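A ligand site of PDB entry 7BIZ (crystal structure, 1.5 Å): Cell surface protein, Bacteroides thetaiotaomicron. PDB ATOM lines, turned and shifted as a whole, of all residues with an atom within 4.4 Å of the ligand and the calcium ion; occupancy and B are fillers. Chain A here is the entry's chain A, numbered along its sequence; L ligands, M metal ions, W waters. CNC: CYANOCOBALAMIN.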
ATOM      1  N   GLN A 233      19.152  -9.806  33.531  1.00  0.00           N
ATOM      2  CA  GLN A 233      19.509 -11.067  32.883  1.00  0.00           C
ATOM      3  C   GLN A 233      20.972 -11.154  32.474  1.00  0.00           C
ATOM      4  O   GLN A 233      21.475 -12.266  32.275  1.00  0.00           O
ATOM      5  CB  GLN A 233      18.625 -11.274  31.668  1.00  0.00           C
ATOM      6  CG  GLN A 233      18.948 -10.266  30.562  1.00  0.00           C
ATOM      7  CD  GLN A 233      17.807 -10.108  29.594  1.00  0.00           C
ATOM      8  OE1 GLN A 233      17.314 -11.082  29.036  1.00  0.00           O
ATOM      9  NE2 GLN A 233      17.374  -8.847  29.374  1.00  0.00           N
ATOM     10  N   PHE A 234      21.664 -10.019  32.332  1.00  0.00           N
ATOM     11  CA  PHE A 234      23.078 -10.069  31.990  1.00  0.00           C
ATOM     12  C   PHE A 234      23.977 -10.021  33.210  1.00  0.00           C
ATOM     13  O   PHE A 234      25.200 -10.139  33.064  1.00  0.00           O
ATOM     14  CB  PHE A 234      23.402  -8.935  31.019  1.00  0.00           C
ATOM     15  CG  PHE A 234      22.711  -9.112  29.713  1.00  0.00           C
ATOM     16  CD1 PHE A 234      23.145 -10.086  28.824  1.00  0.00           C
ATOM     17  CD2 PHE A 234      21.579  -8.357  29.408  1.00  0.00           C
ATOM     18  CE1 PHE A 234      22.455 -10.308  27.602  1.00  0.00           C
ATOM     19  CE2 PHE A 234      20.881  -8.569  28.193  1.00  0.00           C
ATOM     20  CZ  PHE A 234      21.327  -9.540  27.311  1.00  0.00           C
ATOM     21  N   ILE A 241      28.070 -14.434  25.564  1.00  0.00           N
ATOM     22  CA  ILE A 241      27.228 -13.257  25.430  1.00  0.00           C
ATOM     23  C   ILE A 241      27.293 -12.374  26.668  1.00  0.00           C
ATOM     24  O   ILE A 241      27.231 -11.144  26.569  1.00  0.00           O
ATOM     25  CB  ILE A 241      25.774 -13.705  25.111  1.00  0.00           C
ATOM     26  CG1 ILE A 241      25.640 -13.984  23.606  1.00  0.00           C
ATOM     27  CG2 ILE A 241      24.743 -12.684  25.612  1.00  0.00           C
ATOM     28  CD1 ILE A 241      24.227 -14.386  23.187  1.00  0.00           C
ATOM     29  N   HIS A 267      30.017  -4.805  26.457  1.00  0.00           N
ATOM     30  CA  HIS A 267      28.930  -4.211  27.225  1.00  0.00           C
ATOM     31  C   HIS A 267      29.106  -4.380  28.717  1.00  0.00           C
ATOM     32  O   HIS A 267      29.627  -5.386  29.204  1.00  0.00           O
ATOM     33  CB  HIS A 267      27.545  -4.768  26.846  1.00  0.00           C
ATOM     34  CG  HIS A 267      27.254  -6.172  27.296  1.00  0.00           C
ATOM     35  ND1 HIS A 267      26.911  -6.510  28.593  1.00  0.00           N
ATOM     36  CD2 HIS A 267      27.151  -7.323  26.581  1.00  0.00           C
ATOM     37  CE1 HIS A 267      26.668  -7.810  28.660  1.00  0.00           C
ATOM     38  NE2 HIS A 267      26.792  -8.315  27.454  1.00  0.00           N
ATOM     39  N   ASN A 299      24.239   0.765  22.910  1.00  0.00           N
ATOM     40  CA  ASN A 299      23.975  -0.095  21.758  1.00  0.00           C
ATOM     41  C   ASN A 299      22.546   0.084  21.261  1.00  0.00           C
ATOM     42  O   ASN A 299      21.867  -0.863  20.823  1.00  0.00           O
ATOM     43  CB  ASN A 299      24.297  -1.565  22.072  1.00  0.00           C
ATOM     44  CG  ASN A 299      23.507  -2.123  23.256  1.00  0.00           C
ATOM     45  OD1 ASN A 299      22.748  -1.398  23.920  1.00  0.00           O
ATOM     46  ND2 ASN A 299      23.655  -3.430  23.499  1.00  0.00           N
ATOM     47  N   PHE A 301      19.264   1.034  19.048  1.00  0.00           N
ATOM     48  CA  PHE A 301      18.733   1.148  17.696  1.00  0.00           C
ATOM     49  C   PHE A 301      17.229   1.373  17.860  1.00  0.00           C
ATOM     50  O   PHE A 301      16.707   1.333  18.990  1.00  0.00           O
ATOM     51  CB  PHE A 301      19.094  -0.069  16.822  1.00  0.00           C
ATOM     52  CG  PHE A 301      18.676  -1.390  17.391  1.00  0.00           C
ATOM     53  CD1 PHE A 301      17.424  -1.899  17.106  1.00  0.00           C
ATOM     54  CD2 PHE A 301      19.542  -2.123  18.187  1.00  0.00           C
ATOM     55  CE1 PHE A 301      17.017  -3.142  17.626  1.00  0.00           C
ATOM     56  CE2 PHE A 301      19.157  -3.365  18.712  1.00  0.00           C
ATOM     57  CZ  PHE A 301      17.887  -3.869  18.443  1.00  0.00           C
ATOM     58  N   ASP A 302      16.535   1.647  16.749  1.00  0.00           N
ATOM     59  CA  ASP A 302      15.116   1.987  16.847  1.00  0.00           C
ATOM     60  C   ASP A 302      14.318   0.795  17.389  1.00  0.00           C
ATOM     61  O   ASP A 302      14.273  -0.278  16.778  1.00  0.00           O
ATOM     62  CB  ASP A 302      14.596   2.422  15.469  1.00  0.00           C
ATOM     63  CG  ASP A 302      13.211   3.054  15.520  1.00  0.00           C
ATOM     64  OD1 ASP A 302      12.651   3.306  16.611  1.00  0.00           O
ATOM     65  OD2 ASP A 302      12.658   3.308  14.410  1.00  0.00           O
ATOM     66  N   GLY A 303      13.686   0.973  18.560  1.00  0.00           N
ATOM     67  CA  GLY A 303      13.018  -0.117  19.232  1.00  0.00           C
ATOM     68  C   GLY A 303      13.805  -0.678  20.400  1.00  0.00           C
ATOM     69  O   GLY A 303      13.269  -1.483  21.169  1.00  0.00           O
ATOM     70  N   SER A 304      15.066  -0.260  20.556  1.00  0.00           N
ATOM     71  CA  SER A 304      15.929  -0.763  21.616  1.00  0.00           C
ATOM     72  C   SER A 304      16.537   0.428  22.356  1.00  0.00           C
ATOM     73  O   SER A 304      17.746   0.625  22.341  1.00  0.00           O
ATOM     74  CB  SER A 304      17.013  -1.667  21.044  1.00  0.00           C
ATOM     75  OG  SER A 304      17.660  -2.399  22.096  1.00  0.00           O
ATOM     76  N   GLU A 306      17.014   2.003  26.090  1.00  0.00           N
ATOM     77  CA  GLU A 306      17.045   1.575  27.492  1.00  0.00           C
ATOM     78  C   GLU A 306      17.734   2.682  28.270  1.00  0.00           C
ATOM     79  O   GLU A 306      18.926   2.604  28.594  1.00  0.00           O
ATOM     80  CB  GLU A 306      17.785   0.229  27.636  1.00  0.00           C
ATOM     81  CG  GLU A 306      17.227  -0.881  26.761  1.00  0.00           C
ATOM     82  CD  GLU A 306      17.903  -2.208  27.006  1.00  0.00           C
ATOM     83  OE1 GLU A 306      17.334  -3.047  27.762  1.00  0.00           O
ATOM     84  OE2 GLU A 306      19.022  -2.413  26.482  1.00  0.00           O
ATOM     85  N   LEU A 372      14.715 -15.818  32.737  1.00  0.00           N
ATOM     86  CA  LEU A 372      14.508 -16.289  31.353  1.00  0.00           C
ATOM     87  C   LEU A 372      15.407 -17.498  31.075  1.00  0.00           C
ATOM     88  O   LEU A 372      16.529 -17.387  30.589  1.00  0.00           O
ATOM     89  CB  LEU A 372      14.779 -15.153  30.356  1.00  0.00           C
ATOM     90  CG  LEU A 372      13.883 -13.915  30.494  1.00  0.00           C
ATOM     91  CD1 LEU A 372      14.297 -12.919  29.398  1.00  0.00           C
ATOM     92  CD2 LEU A 372      12.405 -14.260  30.368  1.00  0.00           C
ATOM     93  N   TYR A 375      17.278 -18.134  27.752  1.00  0.00           N
ATOM     94  CA  TYR A 375      18.376 -17.306  27.259  1.00  0.00           C
ATOM     95  C   TYR A 375      19.520 -17.110  28.245  1.00  0.00           C
ATOM     96  O   TYR A 375      20.676 -17.031  27.821  1.00  0.00           O
ATOM     97  CB  TYR A 375      17.858 -15.917  26.832  1.00  0.00           C
ATOM     98  CG  TYR A 375      16.706 -16.006  25.876  1.00  0.00           C
ATOM     99  CD1 TYR A 375      16.875 -16.561  24.605  1.00  0.00           C
ATOM    100  CD2 TYR A 375      15.440 -15.573  26.245  1.00  0.00           C
ATOM    101  CE1 TYR A 375      15.795 -16.665  23.723  1.00  0.00           C
ATOM    102  CE2 TYR A 375      14.371 -15.680  25.392  1.00  0.00           C
ATOM    103  CZ  TYR A 375      14.552 -16.231  24.127  1.00  0.00           C
ATOM    104  OH  TYR A 375      13.472 -16.335  23.274  1.00  0.00           O
ATOM    105  N   HIS A 376      19.242 -17.025  29.544  1.00  0.00           N
ATOM    106  CA  HIS A 376      20.293 -16.646  30.500  1.00  0.00           C
ATOM    107  C   HIS A 376      20.126 -17.532  31.721  1.00  0.00           C
ATOM    108  O   HIS A 376      19.232 -17.313  32.542  1.00  0.00           O
ATOM    109  CB  HIS A 376      20.234 -15.151  30.828  1.00  0.00           C
ATOM    110  CG  HIS A 376      20.244 -14.299  29.604  1.00  0.00           C
ATOM    111  ND1 HIS A 376      21.340 -14.195  28.780  1.00  0.00           N
ATOM    112  CD2 HIS A 376      19.266 -13.547  29.025  1.00  0.00           C
ATOM    113  CE1 HIS A 376      21.058 -13.402  27.765  1.00  0.00           C
ATOM    114  NE2 HIS A 376      19.806 -12.995  27.885  1.00  0.00           N
ATOM    115  N   TYR A 410       5.628  -8.517  18.807  1.00  0.00           N
ATOM    116  CA  TYR A 410       6.975  -8.000  19.038  1.00  0.00           C
ATOM    117  C   TYR A 410       6.939  -6.784  19.950  1.00  0.00           C
ATOM    118  O   TYR A 410       5.969  -6.019  19.993  1.00  0.00           O
ATOM    119  CB  TYR A 410       7.669  -7.605  17.728  1.00  0.00           C
ATOM    120  CG  TYR A 410       7.888  -8.766  16.789  1.00  0.00           C
ATOM    121  CD1 TYR A 410       8.460  -9.942  17.224  1.00  0.00           C
ATOM    122  CD2 TYR A 410       7.504  -8.681  15.445  1.00  0.00           C
ATOM    123  CE1 TYR A 410       8.658 -11.008  16.371  1.00  0.00           C
ATOM    124  CE2 TYR A 410       7.694  -9.744  14.593  1.00  0.00           C
ATOM    125  CZ  TYR A 410       8.270 -10.907  15.056  1.00  0.00           C
ATOM    126  OH  TYR A 410       8.466 -11.986  14.217  1.00  0.00           O
ATOM    127  N   TRP A 411       8.046  -6.600  20.647  1.00  0.00           N
ATOM    128  CA  TRP A 411       8.206  -5.539  21.614  1.00  0.00           C
ATOM    129  C   TRP A 411       8.977  -4.362  21.024  1.00  0.00           C
ATOM    130  O   TRP A 411       9.908  -4.533  20.230  1.00  0.00           O
ATOM    131  CB  TRP A 411       8.965  -6.062  22.840  1.00  0.00           C
ATOM    132  CG  TRP A 411       8.121  -6.929  23.712  1.00  0.00           C
ATOM    133  CD1 TRP A 411       7.941  -8.278  23.620  1.00  0.00           C
ATOM    134  CD2 TRP A 411       7.324  -6.495  24.821  1.00  0.00           C
ATOM    135  NE1 TRP A 411       7.094  -8.722  24.617  1.00  0.00           N
ATOM    136  CE2 TRP A 411       6.706  -7.645  25.363  1.00  0.00           C
ATOM    137  CE3 TRP A 411       7.076  -5.245  25.401  1.00  0.00           C
ATOM    138  CZ2 TRP A 411       5.849  -7.584  26.478  1.00  0.00           C
ATOM    139  CZ3 TRP A 411       6.239  -5.190  26.530  1.00  0.00           C
ATOM    140  CH2 TRP A 411       5.637  -6.352  27.050  1.00  0.00           C
ATOM    141  N   THR A 434      22.610   1.287  12.686  1.00  0.00           N
ATOM    142  CA  THR A 434      21.176   1.351  12.952  1.00  0.00           C
ATOM    143  C   THR A 434      20.514  -0.001  12.850  1.00  0.00           C
ATOM    144  O   THR A 434      19.319  -0.120  13.155  1.00  0.00           O
ATOM    145  CB  THR A 434      20.507   2.341  12.003  1.00  0.00           C
ATOM    146  OG1 THR A 434      20.731   1.947  10.646  1.00  0.00           O
ATOM    147  CG2 THR A 434      21.048   3.759  12.237  1.00  0.00           C
ATOM    148  N   VAL A 435      21.267  -1.019  12.437  1.00  0.00           N
ATOM    149  CA  VAL A 435      20.742  -2.374  12.408  1.00  0.00           C
ATOM    150  C   VAL A 435      20.862  -3.022  13.777  1.00  0.00           C
ATOM    151  O   VAL A 435      19.887  -3.554  14.318  1.00  0.00           O
ATOM    152  CB  VAL A 435      21.474  -3.202  11.340  1.00  0.00           C
ATOM    153  CG1 VAL A 435      21.015  -4.667  11.435  1.00  0.00           C
ATOM    154  CG2 VAL A 435      21.217  -2.624   9.954  1.00  0.00           C
ATOM    155  N   ASP A 436      22.061  -3.006  14.363  1.00  0.00           N
ATOM    156  CA  ASP A 436      22.269  -3.761  15.593  1.00  0.00           C
ATOM    157  C   ASP A 436      22.817  -2.928  16.749  1.00  0.00           C
ATOM    158  O   ASP A 436      23.109  -3.487  17.808  1.00  0.00           O
ATOM    159  CB  ASP A 436      23.178  -4.974  15.329  1.00  0.00           C
ATOM    160  CG  ASP A 436      24.643  -4.625  15.073  1.00  0.00           C
ATOM    161  OD1 ASP A 436      25.034  -3.443  15.155  1.00  0.00           O
ATOM    162  OD2 ASP A 436      25.411  -5.567  14.738  1.00  0.00           O
ATOM    163  N   TRP A 477       9.993 -11.566  26.301  1.00  0.00           N
ATOM    164  CA  TRP A 477      11.183 -12.362  26.001  1.00  0.00           C
ATOM    165  C   TRP A 477      12.452 -11.526  25.814  1.00  0.00           C
ATOM    166  O   TRP A 477      13.536 -12.111  25.705  1.00  0.00           O
ATOM    167  CB  TRP A 477      10.918 -13.251  24.764  1.00  0.00           C
ATOM    168  CG  TRP A 477      10.681 -12.546  23.435  1.00  0.00           C
ATOM    169  CD1 TRP A 477      10.362 -11.217  23.212  1.00  0.00           C
ATOM    170  CD2 TRP A 477      10.759 -13.155  22.146  1.00  0.00           C
ATOM    171  NE1 TRP A 477      10.243 -10.983  21.853  1.00  0.00           N
ATOM    172  CE2 TRP A 477      10.488 -12.158  21.175  1.00  0.00           C
ATOM    173  CE3 TRP A 477      11.031 -14.449  21.713  1.00  0.00           C
ATOM    174  CZ2 TRP A 477      10.477 -12.430  19.807  1.00  0.00           C
ATOM    175  CZ3 TRP A 477      11.042 -14.720  20.365  1.00  0.00           C
ATOM    176  CH2 TRP A 477      10.745 -13.708  19.417  1.00  0.00           C
ATOM    177  N   LEU A 478      12.348 -10.202  25.767  1.00  0.00           N
ATOM    178  CA  LEU A 478      13.542  -9.366  25.802  1.00  0.00           C
ATOM    179  C   LEU A 478      14.094  -9.213  27.206  1.00  0.00           C
ATOM    180  O   LEU A 478      15.198  -8.659  27.369  1.00  0.00           O
ATOM    181  CB  LEU A 478      13.263  -7.967  25.246  1.00  0.00           C
ATOM    182  CG  LEU A 478      12.618  -7.878  23.870  1.00  0.00           C
ATOM    183  CD1 LEU A 478      12.634  -6.407  23.360  1.00  0.00           C
ATOM    184  CD2 LEU A 478      13.364  -8.813  22.899  1.00  0.00           C
ATOM    185  N   GLY A 479      13.354  -9.616  28.227  1.00  0.00           N
ATOM    186  CA  GLY A 479      13.885  -9.420  29.568  1.00  0.00           C
ATOM    187  C   GLY A 479      13.732  -7.977  30.019  1.00  0.00           C
ATOM    188  O   GLY A 479      12.961  -7.199  29.433  1.00  0.00           O
ATOM    189  N   SER A 482      17.253  -2.465  30.495  1.00  0.00           N
ATOM    190  CA  SER A 482      18.529  -2.280  31.207  1.00  0.00           C
ATOM    191  C   SER A 482      19.507  -1.520  30.337  1.00  0.00           C
ATOM    192  O   SER A 482      19.895  -2.000  29.263  1.00  0.00           O
ATOM    193  CB  SER A 482      19.131  -3.628  31.596  1.00  0.00           C
ATOM    194  OG  SER A 482      19.109  -4.524  30.485  1.00  0.00           O
ATOM    195  N   GLU A 484      22.882  -0.420  28.801  1.00  0.00           N
ATOM    196  CA  GLU A 484      24.257  -0.901  28.639  1.00  0.00           C
ATOM    197  C   GLU A 484      25.174   0.254  28.235  1.00  0.00           C
ATOM    198  O   GLU A 484      24.786   1.116  27.429  1.00  0.00           O
ATOM    199  CB  GLU A 484      24.376  -1.995  27.584  1.00  0.00           C
ATOM    200  CG  GLU A 484      24.026  -3.403  28.128  1.00  0.00           C
ATOM    201  CD  GLU A 484      22.524  -3.636  28.146  1.00  0.00           C
ATOM    202  OE1 GLU A 484      22.014  -4.368  29.021  1.00  0.00           O
ATOM    203  OE2 GLU A 484      21.827  -3.095  27.278  1.00  0.00           O
HETATM  204 CO   CNC L   1      16.997 -10.410  18.086  1.00  0.00          CO
HETATM  205  N21 CNC L   1      17.443  -9.018  16.902  1.00  0.00           N
HETATM  206  N22 CNC L   1      15.248 -10.438  17.422  1.00  0.00           N
HETATM  207  N23 CNC L   1      16.610 -11.185  19.742  1.00  0.00           N
HETATM  208  N24 CNC L   1      18.871 -10.407  18.406  1.00  0.00           N
HETATM  209  C1  CNC L   1      18.840  -8.856  16.632  1.00  0.00           C
HETATM  210  C20 CNC L   1      18.897  -7.653  17.626  1.00  0.00           C
HETATM  211  C2  CNC L   1      19.127  -8.147  15.313  1.00  0.00           C
HETATM  212  C25 CNC L   1      19.978  -6.852  15.336  1.00  0.00           C
HETATM  213  C26 CNC L   1      19.862  -9.248  14.560  1.00  0.00           C
HETATM  214  C27 CNC L   1      19.916  -9.075  13.031  1.00  0.00           C
HETATM  215  O28 CNC L   1      20.794  -8.387  12.532  1.00  0.00           O
HETATM  216  N29 CNC L   1      19.009  -9.696  12.273  1.00  0.00           N
HETATM  217  C3  CNC L   1      17.672  -8.011  14.766  1.00  0.00           C
HETATM  218  C30 CNC L   1      17.005  -6.562  14.868  1.00  0.00           C
HETATM  219  C31 CNC L   1      17.243  -5.675  13.595  1.00  0.00           C
HETATM  220  C32 CNC L   1      16.445  -4.386  13.722  1.00  0.00           C
HETATM  221  O34 CNC L   1      17.014  -3.294  13.959  1.00  0.00           O
HETATM  222  N33 CNC L   1      15.124  -4.416  13.572  1.00  0.00           N
HETATM  223  C4  CNC L   1      16.899  -8.929  15.691  1.00  0.00           C
HETATM  224  C5  CNC L   1      15.569  -9.371  15.297  1.00  0.00           C
HETATM  225  C35 CNC L   1      15.320  -9.298  13.736  1.00  0.00           C
HETATM  226  C6  CNC L   1      14.828 -10.202  16.116  1.00  0.00           C
HETATM  227  C7  CNC L   1      13.381 -10.638  15.882  1.00  0.00           C
HETATM  228  C36 CNC L   1      12.396  -9.706  15.064  1.00  0.00           C
HETATM  229  C37 CNC L   1      13.533 -12.065  15.289  1.00  0.00           C
HETATM  230  C38 CNC L   1      12.161 -12.775  15.092  1.00  0.00           C
HETATM  231  O39 CNC L   1      11.672 -12.821  13.921  1.00  0.00           O
HETATM  232  N40 CNC L   1      11.545 -13.355  16.086  1.00  0.00           N
HETATM  233  C8  CNC L   1      12.885 -10.781  17.385  1.00  0.00           C
HETATM  234  C41 CNC L   1      12.188  -9.441  17.799  1.00  0.00           C
HETATM  235  C42 CNC L   1      12.164  -9.239  19.344  1.00  0.00           C
HETATM  236  C43 CNC L   1      11.179  -8.189  19.745  1.00  0.00           C
HETATM  237  O44 CNC L   1      10.105  -8.499  20.305  1.00  0.00           O
HETATM  238  N45 CNC L   1      11.453  -6.898  19.464  1.00  0.00           N
HETATM  239  C9  CNC L   1      14.228 -10.957  18.048  1.00  0.00           C
HETATM  240  C10 CNC L   1      14.257 -11.710  19.236  1.00  0.00           C
HETATM  241  C11 CNC L   1      15.480 -11.937  19.903  1.00  0.00           C
HETATM  242  C12 CNC L   1      15.481 -12.918  21.075  1.00  0.00           C
HETATM  243  C46 CNC L   1      14.283 -12.622  22.064  1.00  0.00           C
HETATM  244  C47 CNC L   1      15.353 -14.387  20.585  1.00  0.00           C
HETATM  245  C13 CNC L   1      16.929 -12.697  21.626  1.00  0.00           C
HETATM  246  C48 CNC L   1      16.941 -11.864  22.985  1.00  0.00           C
HETATM  247  C49 CNC L   1      16.787 -12.783  24.234  1.00  0.00           C
HETATM  248  C50 CNC L   1      17.214 -12.098  25.556  1.00  0.00           C
HETATM  249  O51 CNC L   1      16.337 -11.795  26.447  1.00  0.00           O
HETATM  250  N52 CNC L   1      18.467 -11.848  25.731  1.00  0.00           N
HETATM  251  C14 CNC L   1      17.522 -11.925  20.444  1.00  0.00           C
HETATM  252  C15 CNC L   1      18.911 -11.723  20.451  1.00  0.00           C
HETATM  253  C53 CNC L   1      19.785 -12.495  21.466  1.00  0.00           C
HETATM  254  C16 CNC L   1      19.463 -10.805  19.471  1.00  0.00           C
HETATM  255  C17 CNC L   1      21.021 -10.707  19.280  1.00  0.00           C
HETATM  256  C54 CNC L   1      21.664 -11.943  18.543  1.00  0.00           C
HETATM  257  C55 CNC L   1      21.887 -10.316  20.469  1.00  0.00           C
HETATM  258  C56 CNC L   1      21.229  -9.216  21.353  1.00  0.00           C
HETATM  259  C57 CNC L   1      22.068  -9.061  22.618  1.00  0.00           C
HETATM  260  O58 CNC L   1      22.275 -10.030  23.330  1.00  0.00           O
HETATM  261  N59 CNC L   1      22.562  -7.880  22.909  1.00  0.00           N
HETATM  262  C18 CNC L   1      21.026  -9.491  18.336  1.00  0.00           C
HETATM  263  C60 CNC L   1      22.175  -9.388  17.269  1.00  0.00           C
HETATM  264  C61 CNC L   1      23.515  -9.082  17.902  1.00  0.00           C
HETATM  265  O63 CNC L   1      24.456  -9.861  17.767  1.00  0.00           O
HETATM  266  N62 CNC L   1      23.630  -7.964  18.616  1.00  0.00           N
HETATM  267  C19 CNC L   1      19.752  -9.625  17.547  1.00  0.00           C
HETATM  268  C1P CNC L   1      23.393  -7.745  24.139  1.00  0.00           C
HETATM  269  C2P CNC L   1      22.630  -7.026  25.250  1.00  0.00           C
HETATM  270  C3P CNC L   1      23.502  -6.896  26.486  1.00  0.00           C
HETATM  271  O3  CNC L   1      22.226  -5.708  24.811  1.00  0.00           O
HETATM  272  O4  CNC L   1      20.116  -5.476  26.242  1.00  0.00           O
HETATM  273  O5  CNC L   1      20.627  -3.816  24.400  1.00  0.00           O
HETATM  274  P   CNC L   1      20.710  -5.236  24.899  1.00  0.00           P
HETATM  275  O2  CNC L   1      19.974  -6.293  23.862  1.00  0.00           O
HETATM  276  C3R CNC L   1      18.570  -6.335  23.835  1.00  0.00           C
HETATM  277  C2R CNC L   1      17.994  -6.119  22.443  1.00  0.00           C
HETATM  278  O7R CNC L   1      18.841  -6.759  21.514  1.00  0.00           O
HETATM  279  C1R CNC L   1      16.591  -6.803  22.573  1.00  0.00           C
HETATM  280  O6R CNC L   1      16.793  -7.875  23.440  1.00  0.00           O
HETATM  281  C4R CNC L   1      18.140  -7.815  23.992  1.00  0.00           C
HETATM  282  C5R CNC L   1      18.117  -8.294  25.460  1.00  0.00           C
HETATM  283  O8R CNC L   1      17.223  -7.403  26.195  1.00  0.00           O
HETATM  284  N1B CNC L   1      16.283  -7.340  21.256  1.00  0.00           N
HETATM  285  C8B CNC L   1      15.589  -6.667  20.262  1.00  0.00           C
HETATM  286  C2B CNC L   1      16.732  -8.495  20.804  1.00  0.00           C
HETATM  287  N3B CNC L   1      16.332  -8.613  19.529  1.00  0.00           N
HETATM  288  C9B CNC L   1      15.607  -7.501  19.149  1.00  0.00           C
HETATM  289  C4B CNC L   1      14.967  -7.110  17.967  1.00  0.00           C
HETATM  290  C5B CNC L   1      14.291  -5.909  17.897  1.00  0.00           C
HETATM  291  C5M CNC L   1      13.585  -5.484  16.618  1.00  0.00           C
HETATM  292  C6B CNC L   1      14.256  -5.033  19.046  1.00  0.00           C
HETATM  293  C6M CNC L   1      13.542  -3.754  18.972  1.00  0.00           C
HETATM  294  C7B CNC L   1      14.913  -5.436  20.221  1.00  0.00           C
HETATM  295  N1A CNC L   1      17.718 -13.030  16.400  1.00  0.00           N
HETATM  296  C1A CNC L   1      17.439 -12.096  17.006  1.00  0.00           C
HETATM  297 CA    CA M   1      19.689  -4.126  28.132  1.00  0.00          CA
HETATM  298  O   HOH W   1      25.302  -7.166  20.444  1.00  0.00           O
HETATM  299  O   HOH W   2      21.414  -5.764  21.118  1.00  0.00           O
HETATM  300  O   HOH W   3      24.307 -12.271  15.994  1.00  0.00           O
HETATM  301  O   HOH W   4      16.087  -4.830  26.206  1.00  0.00           O
HETATM  302  O   HOH W   5      18.150  -5.944  28.447  1.00  0.00           O
HETATM  303  O   HOH W   6      20.866 -14.634  23.882  1.00  0.00           O
HETATM  304  O   HOH W   7      25.028 -10.611  22.317  1.00  0.00           O
HETATM  305  O   HOH W   8      20.372  -3.114  21.861  1.00  0.00           O
HETATM  306  O   HOH W   9      15.418  -0.752  14.205  1.00  0.00           O
HETATM  307  O   HOH W  10      19.895  -0.553  23.553  1.00  0.00           O
HETATM  308  O   HOH W  11       9.131 -14.489  16.022  1.00  0.00           O
HETATM  309  O   HOH W  12      21.032 -12.157  24.763  1.00  0.00           O
HETATM  310  O   HOH W  13      13.689  -6.282  12.396  1.00  0.00           O
HETATM  311  O   HOH W  14      19.376  -7.468   9.868  1.00  0.00           O
HETATM  312  O   HOH W  15      21.980  -5.938  18.534  1.00  0.00           O
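The backbone carbonyl oxygen (O) of Val 435 lies close to an oxygen (O34) of the ligand (2.9 Å).
Phe 234 touches the ligand.
His 267 touches the ligand (CD2 to C3P, 3.7 Å).
Phe 301 touches the ligand.
O of Gly 303 touches C6M of the ligand, at 3.2 Å.
Ser 304 touches the ligand.
Leu 372 touches the ligand (CD1 to O51, 3.8 Å).
CG of Tyr 375 touches C49 of the ligand, at 3.6 Å.
Asp 436 touches the ligand.
Hydrophobic or aromatic side chains within 4 Å of the ligand: Phe 234, His 267, Phe 301, Leu 372, Tyr 375, His 376, Tyr 410, Trp 411, Val 435, Trp 477 and Leu 478.
Within 4 Å of the ligand: Gln 233, Phe 234, His 267, Asn 299, Phe 301, Gly 303, Ser 304, Glu 306, Leu 372, Tyr 375, His 376, Tyr 410, Trp 411, Val 435, Asp 436, Trp 477, Leu 478 and Glu 484.
Of the 23 residues printed, 3 come within 4 Å of the calcium ion.
The nearest printed residue that does not touch the calcium ion is Phe 234 (4.6 Å).
The backbone carbonyl oxygen (O) of Leu 478 sits at hydrogen-bond distance from an oxygen (O8R) of the ligand (2.7 Å).
A ring nitrogen (NE2) of His 376 sits at hydrogen-bond distance from a nitrogen (N52) of the ligand (2.8 Å).
An oxygen (O44) of the ligand is in hydrogen-bond range of the backbone NH of Trp 411 (2.8 Å).
O of Trp 411 is in hydrogen-bond range of N45 of the ligand.
The side-chain amide oxygen (OE1) of Gln 233 sits close to an oxygen (O51) of the ligand, at 2.9 Å.
The indole nitrogen of Trp 477 is in hydrogen-bond range of an oxygen (O44) of the ligand, 2.9 Å away.
The side-chain amide nitrogen of Asn 299 sits at hydrogen-bond distance from an oxygen (O3) of the ligand.
OH of Tyr 410 is in hydrogen-bond range of O39 of the ligand (3.3 Å).
The calcium ion is bound by O4 of the ligand (2.4 Å), water W5 (2.4 Å), O of Ser 482 (2.4 Å), OG of Ser 482 (2.5 Å), OE2 of Glu 306 (2.5 Å), OE1 of Glu 484 (2.5 Å), OE2 of Glu 484 (2.5 Å) and OE1 of Glu 306 (2.6 Å).
The backbone carbonyl oxygen (O) of Leu 478 sits at hydrogen-bond distance from the side-chain amide nitrogen (NE2) of Gln 233 (3.0 Å).
A ring nitrogen (NE2) of His 376 sits close to the side-chain amide oxygen (OE1) of Gln 233 (3.3 Å).
A ring nitrogen (NE2) of His 267 lies within hydrogen-bond range of the backbone carbonyl oxygen of Ile 241.
Water W5 lies within hydrogen-bond range of an oxygen (O8R) of the ligand (2.8 Å) and the side-chain amide nitrogen of Gln 233 (3.1 Å).
Water W15 lies within hydrogen-bond range of N62 of the ligand and O of Asp 436.
Water W8 lies within hydrogen-bond range of an oxygen (O5) of the ligand, the side-chain hydroxyl (OG) of Ser 304 and the backbone carbonyl oxygen (O) of Asn 299.
Water W12 lies within hydrogen-bond range of a nitrogen (N52) of the ligand and a ring nitrogen (NE2) of His 376.
Water W9 bridges O of Asp 302 and O34 of the ligand.
Water W10 lies within hydrogen-bond range of O of Ser 304, OD1 of Asn 299 and O5 of the ligand.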
